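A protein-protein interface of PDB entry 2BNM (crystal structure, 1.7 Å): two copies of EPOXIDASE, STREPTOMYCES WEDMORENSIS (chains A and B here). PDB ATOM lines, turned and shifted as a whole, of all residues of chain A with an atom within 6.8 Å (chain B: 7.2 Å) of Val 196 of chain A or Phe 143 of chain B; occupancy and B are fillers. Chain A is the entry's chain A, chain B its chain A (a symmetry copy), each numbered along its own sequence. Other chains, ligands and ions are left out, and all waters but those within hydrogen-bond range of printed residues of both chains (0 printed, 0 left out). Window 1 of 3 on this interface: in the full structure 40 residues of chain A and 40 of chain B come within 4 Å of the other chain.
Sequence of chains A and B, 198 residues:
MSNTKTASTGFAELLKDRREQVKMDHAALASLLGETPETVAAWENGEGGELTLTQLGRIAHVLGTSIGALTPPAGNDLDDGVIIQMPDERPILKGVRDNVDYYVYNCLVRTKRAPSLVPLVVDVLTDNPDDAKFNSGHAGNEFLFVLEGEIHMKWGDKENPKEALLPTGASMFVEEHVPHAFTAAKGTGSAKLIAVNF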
ATOM      1  N   LEU A 108       1.181 -16.978 -22.616  1.00  0.00           N
ATOM      2  CA  LEU A 108       0.427 -16.780 -21.405  1.00  0.00           C
ATOM      3  C   LEU A 108       1.379 -16.352 -20.267  1.00  0.00           C
ATOM      4  O   LEU A 108       2.580 -16.130 -20.508  1.00  0.00           O
ATOM      5  CB  LEU A 108      -0.395 -18.028 -21.029  1.00  0.00           C
ATOM      6  CG  LEU A 108      -1.313 -18.549 -22.136  1.00  0.00           C
ATOM      7  CD1 LEU A 108      -1.951 -19.897 -21.691  1.00  0.00           C
ATOM      8  CD2 LEU A 108      -2.359 -17.496 -22.366  1.00  0.00           C
ATOM      9  N   VAL A 109       0.840 -16.239 -19.057  1.00  0.00           N
ATOM     10  CA  VAL A 109       1.602 -15.647 -17.948  1.00  0.00           C
ATOM     11  C   VAL A 109       2.911 -16.382 -17.700  1.00  0.00           C
ATOM     12  O   VAL A 109       2.992 -17.603 -17.833  1.00  0.00           O
ATOM     13  CB  VAL A 109       0.750 -15.604 -16.655  1.00  0.00           C
ATOM     14  CG1 VAL A 109       0.501 -17.018 -16.090  1.00  0.00           C
ATOM     15  CG2 VAL A 109       1.354 -14.625 -15.623  1.00  0.00           C
ATOM     16  N   SER A 116      11.203 -21.906 -15.921  1.00  0.00           N
ATOM     17  CA  SER A 116      10.908 -22.961 -16.890  1.00  0.00           C
ATOM     18  C   SER A 116       9.432 -23.017 -17.329  1.00  0.00           C
ATOM     19  O   SER A 116       9.099 -23.699 -18.305  1.00  0.00           O
ATOM     20  CB  SER A 116      11.391 -24.321 -16.383  1.00  0.00           C
ATOM     21  OG  SER A 116      12.799 -24.272 -16.205  1.00  0.00           O
ATOM     22  N   LEU A 117       8.564 -22.315 -16.617  1.00  0.00           N
ATOM     23  CA  LEU A 117       7.144 -22.292 -16.965  1.00  0.00           C
ATOM     24  C   LEU A 117       6.918 -21.389 -18.190  1.00  0.00           C
ATOM     25  O   LEU A 117       7.068 -20.153 -18.103  1.00  0.00           O
ATOM     26  CB  LEU A 117       6.298 -21.769 -15.791  1.00  0.00           C
ATOM     27  CG  LEU A 117       4.781 -21.605 -16.052  1.00  0.00           C
ATOM     28  CD1 LEU A 117       4.105 -22.989 -16.346  1.00  0.00           C
ATOM     29  CD2 LEU A 117       4.116 -20.954 -14.880  1.00  0.00           C
ATOM     30  N   VAL A 118       6.554 -22.001 -19.309  1.00  0.00           N
ATOM     31  CA  VAL A 118       6.231 -21.228 -20.518  1.00  0.00           C
ATOM     32  C   VAL A 118       4.912 -21.769 -21.064  1.00  0.00           C
ATOM     33  O   VAL A 118       4.924 -22.780 -21.767  1.00  0.00           O
ATOM     34  CB  VAL A 118       7.338 -21.333 -21.587  1.00  0.00           C
ATOM     35  CG1 VAL A 118       7.012 -20.452 -22.857  1.00  0.00           C
ATOM     36  CG2 VAL A 118       8.718 -20.907 -20.976  1.00  0.00           C
ATOM     37  N   PRO A 119       3.797 -21.159 -20.673  1.00  0.00           N
ATOM     38  CA  PRO A 119       2.472 -21.606 -21.163  1.00  0.00           C
ATOM     39  C   PRO A 119       2.055 -20.821 -22.372  1.00  0.00           C
ATOM     40  O   PRO A 119       2.324 -19.619 -22.458  1.00  0.00           O
ATOM     41  CB  PRO A 119       1.545 -21.343 -19.986  1.00  0.00           C
ATOM     42  CG  PRO A 119       2.281 -20.315 -19.102  1.00  0.00           C
ATOM     43  CD  PRO A 119       3.688 -20.069 -19.682  1.00  0.00           C
ATOM     44  N   LEU A 120       1.407 -21.500 -23.304  1.00  0.00           N
ATOM     45  CA  LEU A 120       1.078 -20.857 -24.578  1.00  0.00           C
ATOM     46  C   LEU A 120      -0.302 -21.315 -25.012  1.00  0.00           C
ATOM     47  O   LEU A 120      -0.663 -22.476 -24.781  1.00  0.00           O
ATOM     48  CB  LEU A 120       2.043 -21.327 -25.649  1.00  0.00           C
ATOM     49  CG  LEU A 120       3.542 -21.206 -25.400  1.00  0.00           C
ATOM     50  CD1 LEU A 120       4.325 -22.040 -26.371  1.00  0.00           C
ATOM     51  CD2 LEU A 120       3.941 -19.753 -25.474  1.00  0.00           C
ATOM     52  N   ASN A 141       9.565 -30.873 -19.346  1.00  0.00           N
ATOM     53  CA  ASN A 141       8.318 -31.605 -19.607  1.00  0.00           C
ATOM     54  C   ASN A 141       7.249 -30.665 -20.129  1.00  0.00           C
ATOM     55  O   ASN A 141       7.368 -29.439 -19.984  1.00  0.00           O
ATOM     56  CB  ASN A 141       7.821 -32.255 -18.323  1.00  0.00           C
ATOM     57  CG  ASN A 141       8.726 -33.404 -17.831  1.00  0.00           C
ATOM     58  OD1 ASN A 141       9.381 -34.109 -18.614  1.00  0.00           O
ATOM     59  ND2 ASN A 141       8.708 -33.613 -16.510  1.00  0.00           N
ATOM     60  N   GLU A 142       6.206 -31.230 -20.755  1.00  0.00           N
ATOM     61  CA  GLU A 142       5.131 -30.410 -21.340  1.00  0.00           C
ATOM     62  C   GLU A 142       3.784 -31.067 -21.093  1.00  0.00           C
ATOM     63  O   GLU A 142       3.634 -32.270 -21.267  1.00  0.00           O
ATOM     64  CB  GLU A 142       5.377 -30.216 -22.834  1.00  0.00           C
ATOM     65  CG  GLU A 142       4.457 -29.198 -23.486  1.00  0.00           C
ATOM     66  CD  GLU A 142       4.786 -29.018 -24.964  1.00  0.00           C
ATOM     67  OE1 GLU A 142       4.859 -27.867 -25.434  1.00  0.00           O
ATOM     68  OE2 GLU A 142       4.976 -30.028 -25.655  1.00  0.00           O
ATOM     69  N   PHE A 143       2.815 -30.261 -20.673  1.00  0.00           N
ATOM     70  CA  PHE A 143       1.458 -30.709 -20.545  1.00  0.00           C
ATOM     71  C   PHE A 143       0.670 -29.972 -21.615  1.00  0.00           C
ATOM     72  O   PHE A 143       0.843 -28.767 -21.764  1.00  0.00           O
ATOM     73  CB  PHE A 143       0.905 -30.296 -19.187  1.00  0.00           C
ATOM     74  CG  PHE A 143      -0.597 -30.325 -19.126  1.00  0.00           C
ATOM     75  CD1 PHE A 143      -1.272 -31.540 -18.976  1.00  0.00           C
ATOM     76  CD2 PHE A 143      -1.340 -29.139 -19.275  1.00  0.00           C
ATOM     77  CE1 PHE A 143      -2.695 -31.572 -18.947  1.00  0.00           C
ATOM     78  CE2 PHE A 143      -2.739 -29.175 -19.256  1.00  0.00           C
ATOM     79  CZ  PHE A 143      -3.399 -30.408 -19.094  1.00  0.00           C
ATOM     80  N   LEU A 144      -0.217 -30.695 -22.306  1.00  0.00           N
ATOM     81  CA  LEU A 144      -1.072 -30.072 -23.326  1.00  0.00           C
ATOM     82  C   LEU A 144      -2.552 -30.396 -23.175  1.00  0.00           C
ATOM     83  O   LEU A 144      -2.927 -31.441 -22.640  1.00  0.00           O
ATOM     84  CB  LEU A 144      -0.587 -30.462 -24.722  1.00  0.00           C
ATOM     85  CG  LEU A 144       0.876 -30.193 -25.067  1.00  0.00           C
ATOM     86  CD1 LEU A 144       1.703 -31.457 -24.835  1.00  0.00           C
ATOM     87  CD2 LEU A 144       1.018 -29.687 -26.532  1.00  0.00           C
ATOM     88  N   PHE A 145      -3.409 -29.500 -23.679  1.00  0.00           N
ATOM     89  CA  PHE A 145      -4.860 -29.663 -23.564  1.00  0.00           C
ATOM     90  C   PHE A 145      -5.437 -29.120 -24.876  1.00  0.00           C
ATOM     91  O   PHE A 145      -5.042 -28.054 -25.337  1.00  0.00           O
ATOM     92  CB  PHE A 145      -5.381 -28.819 -22.384  1.00  0.00           C
ATOM     93  CG  PHE A 145      -6.885 -28.846 -22.216  1.00  0.00           C
ATOM     94  CD1 PHE A 145      -7.493 -29.865 -21.487  1.00  0.00           C
ATOM     95  CD2 PHE A 145      -7.685 -27.862 -22.788  1.00  0.00           C
ATOM     96  CE1 PHE A 145      -8.890 -29.911 -21.319  1.00  0.00           C
ATOM     97  CE2 PHE A 145      -9.117 -27.891 -22.627  1.00  0.00           C
ATOM     98  CZ  PHE A 145      -9.698 -28.915 -21.869  1.00  0.00           C
ATOM     99  N   ILE A 194      -3.585 -25.572 -25.663  1.00  0.00           N
ATOM    100  CA  ILE A 194      -2.790 -24.900 -24.610  1.00  0.00           C
ATOM    101  C   ILE A 194      -1.587 -25.815 -24.361  1.00  0.00           C
ATOM    102  O   ILE A 194      -1.773 -27.027 -24.133  1.00  0.00           O
ATOM    103  CB  ILE A 194      -3.646 -24.536 -23.379  1.00  0.00           C
ATOM    104  CG1 ILE A 194      -2.830 -23.778 -22.314  1.00  0.00           C
ATOM    105  CG2 ILE A 194      -4.390 -25.736 -22.814  1.00  0.00           C
ATOM    106  CD1 ILE A 194      -3.671 -23.240 -21.183  1.00  0.00           C
ATOM    107  N   ALA A 195      -0.368 -25.260 -24.453  1.00  0.00           N
ATOM    108  CA  ALA A 195       0.861 -26.035 -24.268  1.00  0.00           C
ATOM    109  C   ALA A 195       1.539 -25.425 -23.049  1.00  0.00           C
ATOM    110  O   ALA A 195       1.799 -24.225 -23.026  1.00  0.00           O
ATOM    111  CB  ALA A 195       1.763 -25.928 -25.456  1.00  0.00           C
ATOM    112  N   VAL A 196       1.765 -26.226 -22.023  1.00  0.00           N
ATOM    113  CA  VAL A 196       2.378 -25.713 -20.783  1.00  0.00           C
ATOM    114  C   VAL A 196       3.724 -26.391 -20.588  1.00  0.00           C
ATOM    115  O   VAL A 196       3.777 -27.531 -20.157  1.00  0.00           O
ATOM    116  CB  VAL A 196       1.488 -25.974 -19.540  1.00  0.00           C
ATOM    117  CG1 VAL A 196       2.113 -25.344 -18.285  1.00  0.00           C
ATOM    118  CG2 VAL A 196       0.060 -25.436 -19.749  1.00  0.00           C
ATOM    119  N   ASN A 197       4.810 -25.719 -20.976  1.00  0.00           N
ATOM    120  CA  ASN A 197       6.137 -26.201 -20.651  1.00  0.00           C
ATOM    121  C   ASN A 197       6.428 -25.860 -19.220  1.00  0.00           C
ATOM    122  O   ASN A 197       6.060 -24.782 -18.769  1.00  0.00           O
ATOM    123  CB  ASN A 197       7.212 -25.610 -21.557  1.00  0.00           C
ATOM    124  CG  ASN A 197       7.707 -26.621 -22.578  1.00  0.00           C
ATOM    125  OD1 ASN A 197       8.570 -27.500 -22.289  1.00  0.00           O
ATOM    126  ND2 ASN A 197       7.142 -26.539 -23.769  1.00  0.00           N
ATOM    127  N   PHE A 198       7.048 -26.788 -18.489  1.00  0.00           N
ATOM    128  CA  PHE A 198       7.302 -26.548 -17.061  1.00  0.00           C
ATOM    129  C   PHE A 198       8.560 -27.276 -16.594  1.00  0.00           C
ATOM    130  O   PHE A 198       9.146 -28.004 -17.391  1.00  0.00           O
ATOM    131  CB  PHE A 198       6.082 -26.891 -16.176  1.00  0.00           C
ATOM    132  CG  PHE A 198       5.702 -28.348 -16.184  1.00  0.00           C
ATOM    133  CD1 PHE A 198       6.156 -29.218 -15.173  1.00  0.00           C
ATOM    134  CD2 PHE A 198       4.889 -28.864 -17.196  1.00  0.00           C
ATOM    135  CE1 PHE A 198       5.800 -30.581 -15.178  1.00  0.00           C
ATOM    136  CE2 PHE A 198       4.535 -30.205 -17.210  1.00  0.00           C
ATOM    137  CZ  PHE A 198       4.995 -31.076 -16.206  1.00  0.00           C
ATOM    138  OXT PHE A 198       9.018 -27.115 -15.453  1.00  0.00           O
ATOM    139  N   LEU B 117       2.577 -33.416 -11.110  1.00  0.00           N
ATOM    140  CA  LEU B 117       1.687 -32.874 -12.136  1.00  0.00           C
ATOM    141  C   LEU B 117       0.250 -33.371 -11.899  1.00  0.00           C
ATOM    142  O   LEU B 117      -0.042 -34.572 -12.070  1.00  0.00           O
ATOM    143  CB  LEU B 117       2.142 -33.302 -13.542  1.00  0.00           C
ATOM    144  CG  LEU B 117       1.235 -32.874 -14.721  1.00  0.00           C
ATOM    145  CD1 LEU B 117       1.186 -31.313 -14.858  1.00  0.00           C
ATOM    146  CD2 LEU B 117       1.720 -33.480 -16.000  1.00  0.00           C
ATOM    147  N   LEU B 120      -6.303 -30.311 -13.956  1.00  0.00           N
ATOM    148  CA  LEU B 120      -7.734 -30.524 -13.728  1.00  0.00           C
ATOM    149  C   LEU B 120      -8.514 -29.538 -14.578  1.00  0.00           C
ATOM    150  O   LEU B 120      -8.068 -28.399 -14.759  1.00  0.00           O
ATOM    151  CB  LEU B 120      -8.072 -30.208 -12.284  1.00  0.00           C
ATOM    152  CG  LEU B 120      -7.282 -30.888 -11.173  1.00  0.00           C
ATOM    153  CD1 LEU B 120      -7.485 -30.195  -9.857  1.00  0.00           C
ATOM    154  CD2 LEU B 120      -7.681 -32.341 -11.099  1.00  0.00           C
ATOM    155  N   ASN B 141       3.657 -25.366  -7.143  1.00  0.00           N
ATOM    156  CA  ASN B 141       3.173 -24.211  -7.912  1.00  0.00           C
ATOM    157  C   ASN B 141       1.965 -24.595  -8.744  1.00  0.00           C
ATOM    158  O   ASN B 141       1.712 -25.788  -8.968  1.00  0.00           O
ATOM    159  CB  ASN B 141       4.272 -23.709  -8.838  1.00  0.00           C
ATOM    160  CG  ASN B 141       5.458 -23.071  -8.087  1.00  0.00           C
ATOM    161  OD1 ASN B 141       5.316 -22.491  -6.999  1.00  0.00           O
ATOM    162  ND2 ASN B 141       6.635 -23.145  -8.719  1.00  0.00           N
ATOM    163  N   GLU B 142       1.200 -23.588  -9.192  1.00  0.00           N
ATOM    164  CA  GLU B 142      -0.022 -23.847  -9.972  1.00  0.00           C
ATOM    165  C   GLU B 142      -0.147 -22.830 -11.094  1.00  0.00           C
ATOM    166  O   GLU B 142       0.061 -21.641 -10.887  1.00  0.00           O
ATOM    167  CB  GLU B 142      -1.244 -23.802  -9.058  1.00  0.00           C
ATOM    168  CG  GLU B 142      -2.527 -24.282  -9.717  1.00  0.00           C
ATOM    169  CD  GLU B 142      -3.696 -24.256  -8.737  1.00  0.00           C
ATOM    170  OE1 GLU B 142      -4.459 -25.239  -8.677  1.00  0.00           O
ATOM    171  OE2 GLU B 142      -3.849 -23.255  -8.025  1.00  0.00           O
ATOM    172  N   PHE B 143      -0.475 -23.319 -12.285  1.00  0.00           N
ATOM    173  CA  PHE B 143      -0.776 -22.466 -13.398  1.00  0.00           C
ATOM    174  C   PHE B 143      -2.257 -22.648 -13.678  1.00  0.00           C
ATOM    175  O   PHE B 143      -2.728 -23.781 -13.706  1.00  0.00           O
ATOM    176  CB  PHE B 143      -0.005 -22.932 -14.628  1.00  0.00           C
ATOM    177  CG  PHE B 143      -0.568 -22.399 -15.916  1.00  0.00           C
ATOM    178  CD1 PHE B 143      -0.302 -21.083 -16.308  1.00  0.00           C
ATOM    179  CD2 PHE B 143      -1.412 -23.196 -16.710  1.00  0.00           C
ATOM    180  CE1 PHE B 143      -0.857 -20.568 -17.514  1.00  0.00           C
ATOM    181  CE2 PHE B 143      -1.964 -22.684 -17.890  1.00  0.00           C
ATOM    182  CZ  PHE B 143      -1.676 -21.360 -18.272  1.00  0.00           C
ATOM    183  N   LEU B 144      -2.957 -21.537 -13.930  1.00  0.00           N
ATOM    184  CA  LEU B 144      -4.387 -21.602 -14.268  1.00  0.00           C
ATOM    185  C   LEU B 144      -4.762 -20.825 -15.522  1.00  0.00           C
ATOM    186  O   LEU B 144      -4.106 -19.848 -15.891  1.00  0.00           O
ATOM    187  CB  LEU B 144      -5.225 -21.126 -13.082  1.00  0.00           C
ATOM    188  CG  LEU B 144      -5.000 -21.807 -11.734  1.00  0.00           C
ATOM    189  CD1 LEU B 144      -4.024 -20.984 -10.894  1.00  0.00           C
ATOM    190  CD2 LEU B 144      -6.349 -22.018 -10.986  1.00  0.00           C
ATOM    191  N   PHE B 145      -5.852 -21.245 -16.175  1.00  0.00           N
ATOM    192  CA  PHE B 145      -6.302 -20.618 -17.421  1.00  0.00           C
ATOM    193  C   PHE B 145      -7.833 -20.645 -17.361  1.00  0.00           C
ATOM    194  O   PHE B 145      -8.425 -21.663 -17.018  1.00  0.00           O
ATOM    195  CB  PHE B 145      -5.816 -21.452 -18.622  1.00  0.00           C
ATOM    196  CG  PHE B 145      -6.291 -20.942 -19.966  1.00  0.00           C
ATOM    197  CD1 PHE B 145      -5.577 -19.949 -20.632  1.00  0.00           C
ATOM    198  CD2 PHE B 145      -7.445 -21.448 -20.555  1.00  0.00           C
ATOM    199  CE1 PHE B 145      -6.001 -19.458 -21.882  1.00  0.00           C
ATOM    200  CE2 PHE B 145      -7.894 -20.960 -21.835  1.00  0.00           C
ATOM    201  CZ  PHE B 145      -7.144 -19.977 -22.492  1.00  0.00           C
ATOM    202  N   VAL B 146      -8.459 -19.498 -17.603  1.00  0.00           N
ATOM    203  CA  VAL B 146      -9.940 -19.412 -17.498  1.00  0.00           C
ATOM    204  C   VAL B 146     -10.525 -19.907 -18.821  1.00  0.00           C
ATOM    205  O   VAL B 146     -10.344 -19.299 -19.876  1.00  0.00           O
ATOM    206  CB  VAL B 146     -10.445 -18.000 -17.143  1.00  0.00           C
ATOM    207  CG1 VAL B 146     -12.017 -17.998 -17.026  1.00  0.00           C
ATOM    208  CG2 VAL B 146      -9.871 -17.503 -15.841  1.00  0.00           C
ATOM    209  N   ALA B 170      -7.966 -15.456 -19.458  1.00  0.00           N
ATOM    210  CA  ALA B 170      -6.954 -14.945 -18.509  1.00  0.00           C
ATOM    211  C   ALA B 170      -6.139 -16.131 -18.011  1.00  0.00           C
ATOM    212  O   ALA B 170      -6.623 -17.274 -18.006  1.00  0.00           O
ATOM    213  CB  ALA B 170      -7.605 -14.244 -17.344  1.00  0.00           C
ATOM    214  N   SER B 171      -4.897 -15.851 -17.626  1.00  0.00           N
ATOM    215  CA  SER B 171      -4.028 -16.888 -17.032  1.00  0.00           C
ATOM    216  C   SER B 171      -3.393 -16.363 -15.739  1.00  0.00           C
ATOM    217  O   SER B 171      -3.288 -15.145 -15.535  1.00  0.00           O
ATOM    218  CB  SER B 171      -2.970 -17.390 -18.035  1.00  0.00           C
ATOM    219  OG  SER B 171      -2.108 -16.340 -18.480  1.00  0.00           O
ATOM    220  N   MET B 172      -2.985 -17.279 -14.865  1.00  0.00           N
ATOM    221  CA  MET B 172      -2.526 -16.942 -13.530  1.00  0.00           C
ATOM    222  C   MET B 172      -1.493 -17.965 -13.097  1.00  0.00           C
ATOM    223  O   MET B 172      -1.532 -19.143 -13.504  1.00  0.00           O
ATOM    224  CB  MET B 172      -3.687 -16.917 -12.541  1.00  0.00           C
ATOM    225  CG  MET B 172      -3.303 -16.713 -11.079  1.00  0.00           C
ATOM    226  SD  MET B 172      -4.868 -16.488 -10.245  1.00  0.00           S
ATOM    227  CE  MET B 172      -4.517 -16.694  -8.493  1.00  0.00           C
ATOM    228  N   PHE B 173      -0.564 -17.497 -12.273  1.00  0.00           N
ATOM    229  CA  PHE B 173       0.403 -18.378 -11.629  1.00  0.00           C
ATOM    230  C   PHE B 173       0.234 -18.125 -10.142  1.00  0.00           C
ATOM    231  O   PHE B 173       0.153 -16.969  -9.721  1.00  0.00           O
ATOM    232  CB  PHE B 173       1.838 -18.020 -12.041  1.00  0.00           C
ATOM    233  CG  PHE B 173       2.889 -18.696 -11.191  1.00  0.00           C
ATOM    234  CD1 PHE B 173       3.354 -19.967 -11.528  1.00  0.00           C
ATOM    235  CD2 PHE B 173       3.408 -18.066 -10.070  1.00  0.00           C
ATOM    236  CE1 PHE B 173       4.368 -20.613 -10.746  1.00  0.00           C
ATOM    237  CE2 PHE B 173       4.425 -18.715  -9.267  1.00  0.00           C
ATOM    238  CZ  PHE B 173       4.891 -19.982  -9.632  1.00  0.00           C
ATOM    239  N   VAL B 174       0.168 -19.202  -9.349  1.00  0.00           N
ATOM    240  CA  VAL B 174       0.056 -19.115  -7.881  1.00  0.00           C
ATOM    241  C   VAL B 174       1.218 -19.902  -7.294  1.00  0.00           C
ATOM    242  O   VAL B 174       1.335 -21.104  -7.531  1.00  0.00           O
ATOM    243  CB  VAL B 174      -1.281 -19.701  -7.311  1.00  0.00           C
ATOM    244  CG1 VAL B 174      -1.351 -19.448  -5.798  1.00  0.00           C
ATOM    245  CG2 VAL B 174      -2.482 -19.063  -7.986  1.00  0.00           C
ATOM    246  N   ILE B 194      -8.953 -24.372 -16.140  1.00  0.00           N
ATOM    247  CA  ILE B 194      -7.970 -25.478 -16.135  1.00  0.00           C
ATOM    248  C   ILE B 194      -6.944 -25.108 -15.059  1.00  0.00           C
ATOM    249  O   ILE B 194      -6.410 -23.981 -15.080  1.00  0.00           O
ATOM    250  CB  ILE B 194      -7.415 -25.768 -17.546  1.00  0.00           C
ATOM    251  CG1 ILE B 194      -6.442 -26.964 -17.547  1.00  0.00           C
ATOM    252  CG2 ILE B 194      -6.834 -24.529 -18.207  1.00  0.00           C
ATOM    253  CD1 ILE B 194      -6.026 -27.399 -18.930  1.00  0.00           C
ATOM    254  N   ALA B 195      -6.707 -26.019 -14.102  1.00  0.00           N
ATOM    255  CA  ALA B 195      -5.773 -25.773 -13.001  1.00  0.00           C
ATOM    256  C   ALA B 195      -4.676 -26.816 -13.165  1.00  0.00           C
ATOM    257  O   ALA B 195      -4.964 -28.009 -13.205  1.00  0.00           O
ATOM    258  CB  ALA B 195      -6.434 -25.938 -11.670  1.00  0.00           C
ATOM    259  N   VAL B 196      -3.442 -26.373 -13.323  1.00  0.00           N
ATOM    260  CA  VAL B 196      -2.322 -27.309 -13.533  1.00  0.00           C
ATOM    261  C   VAL B 196      -1.364 -27.194 -12.359  1.00  0.00           C
ATOM    262  O   VAL B 196      -0.585 -26.257 -12.295  1.00  0.00           O
ATOM    263  CB  VAL B 196      -1.555 -27.018 -14.850  1.00  0.00           C
ATOM    264  CG1 VAL B 196      -0.458 -28.069 -15.080  1.00  0.00           C
ATOM    265  CG2 VAL B 196      -2.510 -26.973 -16.057  1.00  0.00           C
ATOM    266  N   ASN B 197      -1.471 -28.105 -11.389  1.00  0.00           N
ATOM    267  CA  ASN B 197      -0.481 -28.190 -10.337  1.00  0.00           C
ATOM    268  C   ASN B 197       0.727 -28.897 -10.877  1.00  0.00           C
ATOM    269  O   ASN B 197       0.580 -29.849 -11.633  1.00  0.00           O
ATOM    270  CB  ASN B 197      -1.001 -28.916  -9.101  1.00  0.00           C
ATOM    271  CG  ASN B 197      -1.304 -27.952  -7.965  1.00  0.00           C
ATOM    272  OD1 ASN B 197      -0.399 -27.505  -7.203  1.00  0.00           O
ATOM    273  ND2 ASN B 197      -2.569 -27.586  -7.863  1.00  0.00           N
ATOM    274  N   PHE B 198       1.919 -28.412 -10.530  1.00  0.00           N
ATOM    275  CA  PHE B 198       3.144 -29.013 -11.079  1.00  0.00           C
ATOM    276  C   PHE B 198       4.311 -28.878 -10.105  1.00  0.00           C
ATOM    277  O   PHE B 198       4.135 -28.249  -9.063  1.00  0.00           O
ATOM    278  CB  PHE B 198       3.500 -28.459 -12.477  1.00  0.00           C
ATOM    279  CG  PHE B 198       3.839 -26.992 -12.494  1.00  0.00           C
ATOM    280  CD1 PHE B 198       5.180 -26.560 -12.438  1.00  0.00           C
ATOM    281  CD2 PHE B 198       2.829 -26.031 -12.566  1.00  0.00           C
ATOM    282  CE1 PHE B 198       5.499 -25.188 -12.455  1.00  0.00           C
ATOM    283  CE2 PHE B 198       3.134 -24.678 -12.581  1.00  0.00           C
ATOM    284  CZ  PHE B 198       4.471 -24.246 -12.516  1.00  0.00           C
ATOM    285  OXT PHE B 198       5.405 -29.418 -10.323  1.00  0.00           O
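OG of Ser 171 of chain B is in hydrogen-bond range of N of Val 109 of chain A, at 3.0 Å.
The backbone carbonyl oxygen of Met 172 of chain B lies within hydrogen-bond range of the backbone NH of Leu 144 of chain B, at 2.8 Å.
O of Pro 119 of chain A is in hydrogen-bond range of N of Leu 108 of chain A.
The backbone carbonyl oxygen (O) of Asn 141 of chain B is in hydrogen-bond range of the backbone NH (N) of Phe 198 of chain B (3.1 Å).
N of Val 196 of chain A sits at hydrogen-bond distance from O of Phe 143 of chain A (2.7 Å).
O of Asn 141 of chain A sits at hydrogen-bond distance from N of Phe 198 of chain A, 3.1 Å away.
The backbone carbonyl oxygen (O) of Phe 143 of chain B sits at hydrogen-bond distance from the backbone NH (N) of Val 196 of chain B.
Phe 143 of chain B touches Leu 108 of chain A.
Phe 145 of chain B touches Leu 108 of chain A.
Leu 108 of chain A touches Ser 171 of chain B (CB to OG, 3.5 Å).
Val 109 of chain A touches Met 172 of chain B.
Val 109 of chain A touches Phe 173 of chain B.
Phe 143 of chain B touches Pro 119 of chain A.
CD1 of Ile 194 of chain B touches CE2 of Phe 143 of chain A, 3.8 Å away.
CE2 of Phe 143 of chain A touches CG2 of Val 196 of chain B, at 3.9 Å.
Val 196 of chain A touches Phe 143 of chain B (CG2 to CE2, 3.9 Å).
Phe 198 of chain A touches Phe 198 of chain B (CB to CD1, 3.9 Å).
Ser 116 of chain A touches none of the printed residues of chain B.
Of the printed residues of chain B, Phe 143 of chain A touches Ile 194 (3.8 Å) and Val 196 (3.9 Å).
Val 196 of chain A touches just one residue of chain B: Phe 143.
Of the printed residues of chain A, Phe 143 of chain B touches Leu 108 (3.7 Å), Pro 119 (3.5 Å), Ile 194 (3.8 Å) and Val 196 (3.9 Å).
Of the printed residues of chain A, Phe 173 of chain B touches Val 109 (3.99 Å) and Leu 117 (3.6 Å).
The nearest printed residue of chain A that does not touch Phe 173 of chain B is Pro 119 of chain A (7.4 Å).
Of the 18 printed residues of chain B, 8 touch a printed residue of chain A.
Printed residues of chain B that touch a printed residue of chain A: Phe 143, Phe 145, Ser 171, Met 172, Phe 173, Ile 194, Val 196 and Phe 198.
Among the printed residues, no Asp or Glu carboxylate lies within 4 Å of a Lys or Arg side-chain nitrogen of the other chain.
Phe 143 of chain A touches Ile 194 of chain B, and with the chains exchanged Ile 194 of chain A touches Phe 143 of chain B.
Phe 143 of chain A touches Val 196 of chain B, and with the chains exchanged Val 196 of chain A touches Phe 143 of chain B.
Phe 145 of chain A touches Ile 194 of chain B, and with the chains exchanged Ile 194 of chain A touches Phe 145 of chain B.
Phe 198 of chain B touches its own counterpart, Phe 198 of chain A.
12 positions are printed for both chains.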
